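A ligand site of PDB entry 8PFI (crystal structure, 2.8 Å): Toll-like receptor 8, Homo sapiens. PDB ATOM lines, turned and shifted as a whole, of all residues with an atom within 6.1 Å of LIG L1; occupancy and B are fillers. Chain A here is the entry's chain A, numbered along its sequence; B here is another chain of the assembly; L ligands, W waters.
Phe 235 touches LIG L1 (CZ to N5, 3.3 Å). CD1 of Phe 320 touches C9 of LIG L1, at 3.8 Å. Tyr 322 touches LIG L1 (CE1 to C21, 3.5 Å). Ile 323 touches LIG L1. Lys 324 touches LIG L1. Ser 326 touches LIG L1. Gly 350 touches LIG L1 (CA to C9, 3.5 Å). Val 352 touches LIG L1 (CG2 to C7, 3.9 Å). Ile 377 touches LIG L1 (CG2 to C12, 3.6 Å). Phe 379 touches LIG L1. Leu 464 touches LIG L1 (CD2 to O2, 3.9 Å). CE2 of Phe 468 of chain B touches C21 of LIG L1, at 3.9 Å. CD1 of Phe 469 of chain B touches C1 of LIG L1, 3.6 Å away. Ser 490 of chain B touches LIG L1. Ala 492 of chain B touches LIG L1 (CB to C4, 3.6 Å). OE1 of Gln 493 of chain B touches C1 of LIG L1, at 3.5 Å. Arg 515 of chain B touches LIG L1 (NE to C16, 3.6 Å). Hydrophobic or aromatic side chains that line LIG L1: Phe 235, Phe 320, Tyr 322, Val 352, Ile 377, Phe 379, Leu 464, Phe 468 of chain B, Phe 469 of chain B and Ala 492 of chain B. The nearest printed residue that does not touch LIG L1 is Val 494 of chain B (4.1 Å).
Water W1 lies within hydrogen-bond range of N8 of LIG L1 (2.7 Å) and NH2 of Arg 403 (3.1 Å).
O of Glu 401 sits close to N of Ile 377, 3.3 Å away. The side-chain carboxylate of Glu 401 lies within salt-bridge range of the guanidinium group of Arg 403. N of Tyr 322 lies close to O of Gly 350 (3.4 Å). O of Ile 377 sits at hydrogen-bond distance from N of Gly 350 (3.0 Å). The backbone NH (N) of Ile 470 of chain B is in hydrogen-bond range of the side-chain amide oxygen (OE1) of Gln 493 of chain B, at 2.9 Å. The backbone NH (N) of Ala 492 of chain B is in hydrogen-bond range of the backbone carbonyl oxygen (O) of Phe 468 of chain B (3.1 Å). The backbone NH (N) of Phe 320 lies within hydrogen-bond range of the backbone carbonyl oxygen (O) of Arg 349 (2.8 Å). The side-chain amide oxygen of Asn 378 sits at hydrogen-bond distance from the backbone NH of Val 352 (2.8 Å).
The backbone NH of Gly 325 is in hydrogen-bond range of a nitrogen (N3) of LIG L1. OE1 of Glu 401 lies within salt-bridge range of N8 of LIG L1, at 3.8 Å.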
ATOM      1  N   PHE A 235      20.246   9.799 -28.554  1.00  0.00           N
ATOM      2  CA  PHE A 235      20.344   8.352 -28.470  1.00  0.00           C
ATOM      3  C   PHE A 235      21.568   7.827 -29.225  1.00  0.00           C
ATOM      4  O   PHE A 235      21.446   7.336 -30.343  1.00  0.00           O
ATOM      5  CB  PHE A 235      19.054   7.719 -29.057  1.00  0.00           C
ATOM      6  CG  PHE A 235      18.752   6.350 -28.515  1.00  0.00           C
ATOM      7  CD1 PHE A 235      18.079   6.205 -27.313  1.00  0.00           C
ATOM      8  CD2 PHE A 235      19.171   5.207 -29.174  1.00  0.00           C
ATOM      9  CE1 PHE A 235      17.837   4.937 -26.799  1.00  0.00           C
ATOM     10  CE2 PHE A 235      18.901   3.946 -28.659  1.00  0.00           C
ATOM     11  CZ  PHE A 235      18.232   3.819 -27.479  1.00  0.00           C
ATOM     12  N   PHE A 320      12.461   3.255 -31.393  1.00  0.00           N
ATOM     13  CA  PHE A 320      13.042   4.044 -30.312  1.00  0.00           C
ATOM     14  C   PHE A 320      12.144   5.181 -29.843  1.00  0.00           C
ATOM     15  O   PHE A 320      12.584   6.307 -29.668  1.00  0.00           O
ATOM     16  CB  PHE A 320      14.452   4.540 -30.673  1.00  0.00           C
ATOM     17  CG  PHE A 320      15.332   3.423 -31.176  1.00  0.00           C
ATOM     18  CD1 PHE A 320      15.856   2.483 -30.292  1.00  0.00           C
ATOM     19  CD2 PHE A 320      15.566   3.245 -32.521  1.00  0.00           C
ATOM     20  CE1 PHE A 320      16.628   1.428 -30.754  1.00  0.00           C
ATOM     21  CE2 PHE A 320      16.338   2.190 -32.984  1.00  0.00           C
ATOM     22  CZ  PHE A 320      16.856   1.284 -32.091  1.00  0.00           C
ATOM     23  N   TYR A 322      10.239   4.710 -27.006  1.00  0.00           N
ATOM     24  CA  TYR A 322       9.908   4.313 -25.645  1.00  0.00           C
ATOM     25  C   TYR A 322       9.804   5.463 -24.651  1.00  0.00           C
ATOM     26  O   TYR A 322      10.381   6.525 -24.869  1.00  0.00           O
ATOM     27  CB  TYR A 322      10.909   3.244 -25.137  1.00  0.00           C
ATOM     28  CG  TYR A 322      12.307   3.755 -24.866  1.00  0.00           C
ATOM     29  CD1 TYR A 322      12.648   4.293 -23.634  1.00  0.00           C
ATOM     30  CD2 TYR A 322      13.311   3.623 -25.811  1.00  0.00           C
ATOM     31  CE1 TYR A 322      13.921   4.769 -23.377  1.00  0.00           C
ATOM     32  CE2 TYR A 322      14.611   4.062 -25.551  1.00  0.00           C
ATOM     33  CZ  TYR A 322      14.907   4.625 -24.335  1.00  0.00           C
ATOM     34  OH  TYR A 322      16.186   5.065 -24.069  1.00  0.00           O
ATOM     35  N   ILE A 323       9.078   5.258 -23.552  1.00  0.00           N
ATOM     36  CA  ILE A 323       8.978   6.242 -22.489  1.00  0.00           C
ATOM     37  C   ILE A 323       9.966   5.785 -21.420  1.00  0.00           C
ATOM     38  O   ILE A 323       9.904   4.634 -20.990  1.00  0.00           O
ATOM     39  CB  ILE A 323       7.532   6.327 -21.934  1.00  0.00           C
ATOM     40  CG1 ILE A 323       6.542   6.720 -23.036  1.00  0.00           C
ATOM     41  CG2 ILE A 323       7.458   7.288 -20.757  1.00  0.00           C
ATOM     42  CD1 ILE A 323       5.088   6.491 -22.661  1.00  0.00           C
ATOM     43  N   LYS A 324      10.902   6.654 -21.017  1.00  0.00           N
ATOM     44  CA  LYS A 324      11.917   6.284 -20.029  1.00  0.00           C
ATOM     45  C   LYS A 324      11.279   5.852 -18.704  1.00  0.00           C
ATOM     46  O   LYS A 324      10.338   6.488 -18.231  1.00  0.00           O
ATOM     47  CB  LYS A 324      12.919   7.438 -19.825  1.00  0.00           C
ATOM     48  N   GLY A 325      11.715   4.735 -18.168  1.00  0.00           N
ATOM     49  CA  GLY A 325      11.166   4.202 -16.927  1.00  0.00           C
ATOM     50  C   GLY A 325       9.925   3.344 -17.091  1.00  0.00           C
ATOM     51  O   GLY A 325       9.486   2.716 -16.117  1.00  0.00           O
ATOM     52  N   SER A 326       9.345   3.310 -18.290  1.00  0.00           N
ATOM     53  CA  SER A 326       8.123   2.570 -18.567  1.00  0.00           C
ATOM     54  C   SER A 326       8.383   1.262 -19.313  1.00  0.00           C
ATOM     55  O   SER A 326       8.783   1.273 -20.477  1.00  0.00           O
ATOM     56  CB  SER A 326       7.157   3.449 -19.367  1.00  0.00           C
ATOM     57  OG  SER A 326       5.978   2.775 -19.766  1.00  0.00           O
ATOM     58  N   TYR A 327       8.127   0.133 -18.643  1.00  0.00           N
ATOM     59  CA  TYR A 327       8.302  -1.215 -19.189  1.00  0.00           C
ATOM     60  C   TYR A 327       6.934  -1.896 -19.142  1.00  0.00           C
ATOM     61  O   TYR A 327       6.661  -2.672 -18.221  1.00  0.00           O
ATOM     62  CB  TYR A 327       9.307  -1.970 -18.310  1.00  0.00           C
ATOM     63  CG  TYR A 327       9.911  -3.227 -18.909  1.00  0.00           C
ATOM     64  CD1 TYR A 327       9.885  -3.449 -20.280  1.00  0.00           C
ATOM     65  CD2 TYR A 327      10.583  -4.147 -18.110  1.00  0.00           C
ATOM     66  CE1 TYR A 327      10.475  -4.586 -20.841  1.00  0.00           C
ATOM     67  CE2 TYR A 327      11.175  -5.277 -18.665  1.00  0.00           C
ATOM     68  CZ  TYR A 327      11.122  -5.494 -20.018  1.00  0.00           C
ATOM     69  OH  TYR A 327      11.702  -6.614 -20.549  1.00  0.00           O
ATOM     70  N   ARG A 349      11.314  -1.295 -33.429  1.00  0.00           N
ATOM     71  CA  ARG A 349      12.427  -1.500 -32.492  1.00  0.00           C
ATOM     72  C   ARG A 349      12.339  -0.505 -31.335  1.00  0.00           C
ATOM     73  O   ARG A 349      11.708   0.525 -31.471  1.00  0.00           O
ATOM     74  CB  ARG A 349      13.770  -1.338 -33.196  1.00  0.00           C
ATOM     75  CG  ARG A 349      13.999  -2.324 -34.312  1.00  0.00           C
ATOM     76  CD  ARG A 349      15.462  -2.699 -34.483  1.00  0.00           C
ATOM     77  NE  ARG A 349      16.295  -1.534 -34.776  1.00  0.00           N
ATOM     78  CZ  ARG A 349      17.613  -1.582 -34.940  1.00  0.00           C
ATOM     79  NH1 ARG A 349      18.262  -2.742 -34.877  1.00  0.00           N
ATOM     80  NH2 ARG A 349      18.303  -0.470 -35.190  1.00  0.00           N
ATOM     81  N   GLY A 350      12.957  -0.815 -30.214  1.00  0.00           N
ATOM     82  CA  GLY A 350      13.001   0.094 -29.076  1.00  0.00           C
ATOM     83  C   GLY A 350      11.705   0.641 -28.499  1.00  0.00           C
ATOM     84  O   GLY A 350      11.714   1.756 -27.970  1.00  0.00           O
ATOM     85  N   TYR A 351      10.604  -0.100 -28.591  1.00  0.00           N
ATOM     86  CA  TYR A 351       9.350   0.314 -27.931  1.00  0.00           C
ATOM     87  C   TYR A 351       9.461  -0.018 -26.422  1.00  0.00           C
ATOM     88  O   TYR A 351       8.927   0.702 -25.591  1.00  0.00           O
ATOM     89  CB  TYR A 351       8.127  -0.370 -28.574  1.00  0.00           C
ATOM     90  CG  TYR A 351       6.779   0.021 -27.985  1.00  0.00           C
ATOM     91  CD1 TYR A 351       6.266  -0.625 -26.873  1.00  0.00           C
ATOM     92  CD2 TYR A 351       5.958   0.946 -28.632  1.00  0.00           C
ATOM     93  CE1 TYR A 351       5.021  -0.280 -26.340  1.00  0.00           C
ATOM     94  CE2 TYR A 351       4.708   1.269 -28.135  1.00  0.00           C
ATOM     95  CZ  TYR A 351       4.240   0.656 -26.981  1.00  0.00           C
ATOM     96  OH  TYR A 351       3.004   0.974 -26.467  1.00  0.00           O
ATOM     97  N   VAL A 352      10.187  -1.125 -26.083  1.00  0.00           N
ATOM     98  CA  VAL A 352      10.464  -1.653 -24.757  1.00  0.00           C
ATOM     99  C   VAL A 352       9.174  -2.130 -24.076  1.00  0.00           C
ATOM    100  O   VAL A 352       8.442  -1.338 -23.506  1.00  0.00           O
ATOM    101  CB  VAL A 352      11.301  -0.695 -23.861  1.00  0.00           C
ATOM    102  CG1 VAL A 352      11.751  -1.405 -22.595  1.00  0.00           C
ATOM    103  CG2 VAL A 352      12.503  -0.155 -24.635  1.00  0.00           C
ATOM    104  N   ILE A 377      15.558  -5.273 -30.402  1.00  0.00           N
ATOM    105  CA  ILE A 377      15.860  -4.439 -29.224  1.00  0.00           C
ATOM    106  C   ILE A 377      14.593  -3.998 -28.498  1.00  0.00           C
ATOM    107  O   ILE A 377      14.282  -2.804 -28.484  1.00  0.00           O
ATOM    108  CB  ILE A 377      16.790  -3.236 -29.560  1.00  0.00           C
ATOM    109  CG1 ILE A 377      17.869  -3.582 -30.608  1.00  0.00           C
ATOM    110  CG2 ILE A 377      17.454  -2.687 -28.300  1.00  0.00           C
ATOM    111  CD1 ILE A 377      18.400  -2.430 -31.312  1.00  0.00           C
ATOM    112  N   ASN A 378      13.839  -4.951 -27.958  1.00  0.00           N
ATOM    113  CA  ASN A 378      12.586  -4.630 -27.253  1.00  0.00           C
ATOM    114  C   ASN A 378      12.485  -5.222 -25.844  1.00  0.00           C
ATOM    115  O   ASN A 378      11.524  -4.927 -25.136  1.00  0.00           O
ATOM    116  CB  ASN A 378      11.379  -5.050 -28.085  1.00  0.00           C
ATOM    117  CG  ASN A 378      10.744  -3.923 -28.839  1.00  0.00           C
ATOM    118  OD1 ASN A 378      10.269  -2.945 -28.268  1.00  0.00           O
ATOM    119  ND2 ASN A 378      10.703  -4.037 -30.145  1.00  0.00           N
ATOM    120  N   PHE A 379      13.465  -6.067 -25.452  1.00  0.00           N
ATOM    121  CA  PHE A 379      13.527  -6.673 -24.125  1.00  0.00           C
ATOM    122  C   PHE A 379      12.295  -7.531 -23.849  1.00  0.00           C
ATOM    123  O   PHE A 379      11.816  -7.563 -22.715  1.00  0.00           O
ATOM    124  CB  PHE A 379      13.729  -5.588 -23.038  1.00  0.00           C
ATOM    125  CG  PHE A 379      14.857  -4.617 -23.352  1.00  0.00           C
ATOM    126  CD1 PHE A 379      14.591  -3.395 -23.938  1.00  0.00           C
ATOM    127  CD2 PHE A 379      16.166  -4.971 -23.104  1.00  0.00           C
ATOM    128  CE1 PHE A 379      15.634  -2.529 -24.259  1.00  0.00           C
ATOM    129  CE2 PHE A 379      17.202  -4.080 -23.406  1.00  0.00           C
ATOM    130  CZ  PHE A 379      16.924  -2.877 -23.982  1.00  0.00           C
ATOM    131  N   GLU A 401      18.012  -9.380 -30.216  1.00  0.00           N
ATOM    132  CA  GLU A 401      18.191  -8.545 -29.031  1.00  0.00           C
ATOM    133  C   GLU A 401      16.925  -8.410 -28.166  1.00  0.00           C
ATOM    134  O   GLU A 401      16.436  -7.308 -27.909  1.00  0.00           O
ATOM    135  CB  GLU A 401      18.777  -7.167 -29.388  1.00  0.00           C
ATOM    136  CG  GLU A 401      19.504  -6.504 -28.236  1.00  0.00           C
ATOM    137  CD  GLU A 401      20.761  -7.235 -27.796  1.00  0.00           C
ATOM    138  OE1 GLU A 401      20.724  -7.895 -26.722  1.00  0.00           O
ATOM    139  OE2 GLU A 401      21.767  -7.168 -28.535  1.00  0.00           O
ATOM    140  N   ARG A 403      14.657 -10.797 -24.706  1.00  0.00           N
ATOM    141  CA  ARG A 403      14.932 -11.702 -23.581  1.00  0.00           C
ATOM    142  C   ARG A 403      14.104 -12.993 -23.645  1.00  0.00           C
ATOM    143  O   ARG A 403      13.547 -13.423 -22.633  1.00  0.00           O
ATOM    144  CB  ARG A 403      14.761 -11.004 -22.221  1.00  0.00           C
ATOM    145  CG  ARG A 403      15.368  -9.609 -22.131  1.00  0.00           C
ATOM    146  CD  ARG A 403      16.869  -9.612 -22.390  1.00  0.00           C
ATOM    147  NE  ARG A 403      17.307  -8.340 -22.987  1.00  0.00           N
ATOM    148  CZ  ARG A 403      18.297  -8.237 -23.874  1.00  0.00           C
ATOM    149  NH1 ARG A 403      18.954  -9.322 -24.280  1.00  0.00           N
ATOM    150  NH2 ARG A 403      18.622  -7.049 -24.383  1.00  0.00           N
ATOM    151  N   LEU A 464      20.889 -13.141 -30.254  1.00  0.00           N
ATOM    152  CA  LEU A 464      21.098 -12.274 -29.085  1.00  0.00           C
ATOM    153  C   LEU A 464      19.918 -12.297 -28.139  1.00  0.00           C
ATOM    154  O   LEU A 464      19.499 -11.260 -27.638  1.00  0.00           O
ATOM    155  CB  LEU A 464      21.483 -10.848 -29.484  1.00  0.00           C
ATOM    156  CG  LEU A 464      22.858 -10.710 -30.138  1.00  0.00           C
ATOM    157  CD1 LEU A 464      22.883  -9.573 -31.125  1.00  0.00           C
ATOM    158  CD2 LEU A 464      23.936 -10.563 -29.100  1.00  0.00           C
ATOM    159  N   PHE B 468      18.529  -3.868 -17.536  1.00  0.00           N
ATOM    160  CA  PHE B 468      18.933  -2.823 -18.484  1.00  0.00           C
ATOM    161  C   PHE B 468      18.727  -1.396 -17.944  1.00  0.00           C
ATOM    162  O   PHE B 468      19.378  -0.455 -18.420  1.00  0.00           O
ATOM    163  CB  PHE B 468      18.300  -3.029 -19.875  1.00  0.00           C
ATOM    164  CG  PHE B 468      16.793  -2.987 -19.960  1.00  0.00           C
ATOM    165  CD1 PHE B 468      16.032  -4.095 -19.646  1.00  0.00           C
ATOM    166  CD2 PHE B 468      16.145  -1.849 -20.424  1.00  0.00           C
ATOM    167  CE1 PHE B 468      14.651  -4.073 -19.779  1.00  0.00           C
ATOM    168  CE2 PHE B 468      14.762  -1.835 -20.546  1.00  0.00           C
ATOM    169  CZ  PHE B 468      14.027  -2.930 -20.208  1.00  0.00           C
ATOM    170  N   PHE B 469      17.873  -1.225 -16.933  1.00  0.00           N
ATOM    171  CA  PHE B 469      17.656   0.057 -16.264  1.00  0.00           C
ATOM    172  C   PHE B 469      17.163  -0.150 -14.825  1.00  0.00           C
ATOM    173  O   PHE B 469      16.476  -1.129 -14.559  1.00  0.00           O
ATOM    174  CB  PHE B 469      16.723   0.985 -17.084  1.00  0.00           C
ATOM    175  CG  PHE B 469      15.237   0.847 -16.869  1.00  0.00           C
ATOM    176  CD1 PHE B 469      14.582   1.627 -15.930  1.00  0.00           C
ATOM    177  CD2 PHE B 469      14.487  -0.006 -17.648  1.00  0.00           C
ATOM    178  CE1 PHE B 469      13.212   1.519 -15.754  1.00  0.00           C
ATOM    179  CE2 PHE B 469      13.118  -0.106 -17.483  1.00  0.00           C
ATOM    180  CZ  PHE B 469      12.489   0.659 -16.533  1.00  0.00           C
ATOM    181  N   ILE B 470      17.531   0.737 -13.903  1.00  0.00           N
ATOM    182  CA  ILE B 470      17.112   0.599 -12.505  1.00  0.00           C
ATOM    183  C   ILE B 470      15.663   1.058 -12.328  1.00  0.00           C
ATOM    184  O   ILE B 470      15.381   2.254 -12.325  1.00  0.00           O
ATOM    185  CB  ILE B 470      18.085   1.334 -11.545  1.00  0.00           C
ATOM    186  CG1 ILE B 470      19.526   0.845 -11.748  1.00  0.00           C
ATOM    187  CG2 ILE B 470      17.644   1.165 -10.103  1.00  0.00           C
ATOM    188  CD1 ILE B 470      20.561   1.679 -11.082  1.00  0.00           C
ATOM    189  N   SER B 490      24.639  -4.069 -18.664  1.00  0.00           N
ATOM    190  CA  SER B 490      24.319  -3.254 -19.841  1.00  0.00           C
ATOM    191  C   SER B 490      23.387  -2.099 -19.464  1.00  0.00           C
ATOM    192  O   SER B 490      22.582  -1.658 -20.285  1.00  0.00           O
ATOM    193  CB  SER B 490      23.714  -4.107 -20.951  1.00  0.00           C
ATOM    194  OG  SER B 490      24.595  -5.142 -21.360  1.00  0.00           O
ATOM    195  N   ALA B 492      21.850   1.292 -18.947  1.00  0.00           N
ATOM    196  CA  ALA B 492      21.978   2.608 -19.562  1.00  0.00           C
ATOM    197  C   ALA B 492      21.169   3.698 -18.831  1.00  0.00           C
ATOM    198  O   ALA B 492      20.809   4.717 -19.431  1.00  0.00           O
ATOM    199  CB  ALA B 492      21.558   2.536 -21.019  1.00  0.00           C
ATOM    200  N   GLN B 493      20.906   3.495 -17.531  1.00  0.00           N
ATOM    201  CA  GLN B 493      20.135   4.404 -16.691  1.00  0.00           C
ATOM    202  C   GLN B 493      20.675   5.829 -16.662  1.00  0.00           C
ATOM    203  O   GLN B 493      21.875   6.046 -16.488  1.00  0.00           O
ATOM    204  CB  GLN B 493      20.095   3.849 -15.250  1.00  0.00           C
ATOM    205  CG  GLN B 493      19.293   4.679 -14.260  1.00  0.00           C
ATOM    206  CD  GLN B 493      17.812   4.506 -14.447  1.00  0.00           C
ATOM    207  OE1 GLN B 493      17.341   3.457 -14.877  1.00  0.00           O
ATOM    208  NE2 GLN B 493      17.043   5.528 -14.120  1.00  0.00           N
ATOM    209  N   VAL B 494      19.773   6.795 -16.796  1.00  0.00           N
ATOM    210  CA  VAL B 494      20.127   8.192 -16.630  1.00  0.00           C
ATOM    211  C   VAL B 494      19.890   8.402 -15.132  1.00  0.00           C
ATOM    212  O   VAL B 494      18.752   8.385 -14.678  1.00  0.00           O
ATOM    213  CB  VAL B 494      19.239   9.127 -17.473  1.00  0.00           C
ATOM    214  CG1 VAL B 494      19.533  10.590 -17.146  1.00  0.00           C
ATOM    215  CG2 VAL B 494      19.439   8.854 -18.964  1.00  0.00           C
ATOM    216  N   ARG B 515      26.613   1.243 -19.047  1.00  0.00           N
ATOM    217  CA  ARG B 515      26.527   2.366 -19.982  1.00  0.00           C
ATOM    218  C   ARG B 515      25.735   3.504 -19.328  1.00  0.00           C
ATOM    219  O   ARG B 515      24.911   4.147 -19.973  1.00  0.00           O
ATOM    220  CB  ARG B 515      25.821   1.919 -21.287  1.00  0.00           C
ATOM    221  CG  ARG B 515      26.235   0.533 -21.784  1.00  0.00           C
ATOM    222  CD  ARG B 515      25.283   0.010 -22.827  1.00  0.00           C
ATOM    223  NE  ARG B 515      25.502   0.686 -24.104  1.00  0.00           N
ATOM    224  CZ  ARG B 515      26.247   0.187 -25.087  1.00  0.00           C
ATOM    225  NH1 ARG B 515      26.823  -1.006 -24.963  1.00  0.00           N
ATOM    226  NH2 ARG B 515      26.415   0.881 -26.211  1.00  0.00           N
HETATM  227  C1  LIG L   1      15.199   4.902 -17.241  1.00  0.00           C
HETATM  228  C2  LIG L   1      15.205   3.511 -19.341  1.00  0.00           C
HETATM  229  C3  LIG L   1      18.028   2.246 -22.356  1.00  0.00           C
HETATM  230  C4  LIG L   1      18.975   1.279 -23.119  1.00  0.00           C
HETATM  231  C5  LIG L   1      18.399   1.037 -24.484  1.00  0.00           C
HETATM  232  C6  LIG L   1      17.088   1.028 -24.712  1.00  0.00           C
HETATM  233  C7  LIG L   1      16.042   1.271 -23.649  1.00  0.00           C
HETATM  234  C8  LIG L   1      16.941   0.759 -26.133  1.00  0.00           C
HETATM  235  C9  LIG L   1      15.682   0.652 -26.924  1.00  0.00           C
HETATM  236  C10 LIG L   1      20.486   0.665 -25.815  1.00  0.00           C
HETATM  237  C11 LIG L   1      21.086  -0.766 -25.575  1.00  0.00           C
HETATM  238  C12 LIG L   1      20.476  -1.829 -26.561  1.00  0.00           C
HETATM  239  C13 LIG L   1      21.055  -3.260 -26.298  1.00  0.00           C
HETATM  240  C14 LIG L   1      22.165  -3.230 -25.165  1.00  0.00           C
HETATM  241  C15 LIG L   1      23.257  -2.187 -25.583  1.00  0.00           C
HETATM  242  C16 LIG L   1      22.633  -0.763 -25.823  1.00  0.00           C
HETATM  243  C17 LIG L   1      21.445  -2.716 -23.874  1.00  0.00           C
HETATM  244  N1  LIG L   1      15.815   4.282 -18.406  1.00  0.00           N
HETATM  245  N2  LIG L   1      17.111   4.427 -18.758  1.00  0.00           N
HETATM  246  C18 LIG L   1      17.371   3.799 -19.819  1.00  0.00           C
HETATM  247  C19 LIG L   1      16.109   3.124 -20.334  1.00  0.00           C
HETATM  248  C20 LIG L   1      15.738   2.301 -21.424  1.00  0.00           C
HETATM  249  C21 LIG L   1      14.391   1.917 -21.419  1.00  0.00           C
HETATM  250  C22 LIG L   1      13.495   2.367 -20.457  1.00  0.00           C
HETATM  251  C23 LIG L   1      12.040   1.934 -20.519  1.00  0.00           C
HETATM  252  N3  LIG L   1      13.909   3.133 -19.423  1.00  0.00           N
HETATM  253  N4  LIG L   1      16.592   1.924 -22.444  1.00  0.00           N
HETATM  254  N5  LIG L   1      18.116   0.632 -26.586  1.00  0.00           N
HETATM  255  N6  LIG L   1      19.039   0.775 -25.605  1.00  0.00           N
HETATM  256  N7  LIG L   1      22.759  -4.540 -24.876  1.00  0.00           N
HETATM  257  C24 LIG L   1      20.862  -1.274 -24.101  1.00  0.00           C
HETATM  258  C25 LIG L   1      23.385  -5.387 -25.728  1.00  0.00           C
HETATM  259  O1  LIG L   1      23.534  -5.210 -26.931  1.00  0.00           O
HETATM  260  C26 LIG L   1      23.981  -6.662 -25.135  1.00  0.00           C
HETATM  261  C27 LIG L   1      24.059  -7.792 -26.192  1.00  0.00           C
HETATM  262  O2  LIG L   1      24.519  -8.999 -25.542  1.00  0.00           O
HETATM  263  C28 LIG L   1      23.733  -9.511 -24.425  1.00  0.00           C
HETATM  264  C29 LIG L   1      23.676  -8.414 -23.319  1.00  0.00           C
HETATM  265  N8  LIG L   1      23.234  -7.139 -23.929  1.00  0.00           N
HETATM  266  C1  LG2 L   2      19.222 -29.415 -22.376  1.00  0.00           C
HETATM  267  C2  LG2 L   2      20.124 -27.884 -20.598  1.00  0.00           C
HETATM  268  C3  LG2 L   2      23.629 -25.481 -19.870  1.00  0.00           C
HETATM  269  C4  LG2 L   2      24.522 -24.228 -19.734  1.00  0.00           C
HETATM  270  C5  LG2 L   2      24.873 -24.020 -18.289  1.00  0.00           C
HETATM  271  C6  LG2 L   2      24.029 -24.368 -17.317  1.00  0.00           C
HETATM  272  C7  LG2 L   2      22.684 -24.993 -17.532  1.00  0.00           C
HETATM  273  C8  LG2 L   2      24.700 -24.000 -16.081  1.00  0.00           C
HETATM  274  C9  LG2 L   2      24.220 -24.178 -14.681  1.00  0.00           C
HETATM  275  C10 LG2 L   2      27.098 -22.925 -18.476  1.00  0.00           C
HETATM  276  C11 LG2 L   2      26.993 -21.419 -18.879  1.00  0.00           C
HETATM  277  C12 LG2 L   2      26.829 -20.474 -17.639  1.00  0.00           C
HETATM  278  C13 LG2 L   2      26.716 -18.969 -18.072  1.00  0.00           C
HETATM  279  C14 LG2 L   2      26.868 -18.807 -19.635  1.00  0.00           C
HETATM  280  C15 LG2 L   2      28.223 -19.482 -20.065  1.00  0.00           C
HETATM  281  C16 LG2 L   2      28.306 -20.989 -19.621  1.00  0.00           C
HETATM  282  C17 LG2 L   2      25.692 -19.626 -20.259  1.00  0.00           C
HETATM  283  N1  LG2 L   2      20.216 -28.536 -21.782  1.00  0.00           N
HETATM  284  N2  LG2 L   2      21.418 -28.280 -22.316  1.00  0.00           N
HETATM  285  C18 LG2 L   2      22.086 -27.492 -21.577  1.00  0.00           C
HETATM  286  C19 LG2 L   2      21.280 -27.147 -20.345  1.00  0.00           C
HETATM  287  C20 LG2 L   2      21.427 -26.349 -19.186  1.00  0.00           C
HETATM  288  C21 LG2 L   2      20.318 -26.375 -18.305  1.00  0.00           C
HETATM  289  C22 LG2 L   2      19.186 -27.133 -18.589  1.00  0.00           C
HETATM  290  C23 LG2 L   2      18.011 -27.112 -17.617  1.00  0.00           C
HETATM  291  N3  LG2 L   2      19.098 -27.872 -19.709  1.00  0.00           N
HETATM  292  N4  LG2 L   2      22.547 -25.611 -18.875  1.00  0.00           N
HETATM  293  N5  LG2 L   2      25.816 -23.488 -16.418  1.00  0.00           N
HETATM  294  N6  LG2 L   2      25.933 -23.456 -17.770  1.00  0.00           N
HETATM  295  N7  LG2 L   2      26.796 -17.426 -20.123  1.00  0.00           N
HETATM  296  C24 LG2 L   2      25.787 -21.142 -19.856  1.00  0.00           C
HETATM  297  C25 LG2 L   2      27.581 -16.370 -19.752  1.00  0.00           C
HETATM  298  O1  LG2 L   2      28.458 -16.400 -18.900  1.00  0.00           O
HETATM  299  C26 LG2 L   2      27.363 -15.056 -20.493  1.00  0.00           C
HETATM  300  C27 LG2 L   2      27.857 -13.830 -19.663  1.00  0.00           C
HETATM  301  O2  LG2 L   2      26.914 -12.718 -19.641  1.00  0.00           O
HETATM  302  C28 LG2 L   2      26.294 -12.375 -20.911  1.00  0.00           C
HETATM  303  C29 LG2 L   2      25.701 -13.596 -21.683  1.00  0.00           C
HETATM  304  N8  LG2 L   2      25.962 -14.882 -20.956  1.00  0.00           N
HETATM  305  O   HOH W   1      21.055  -6.085 -22.791  1.00  0.00           O
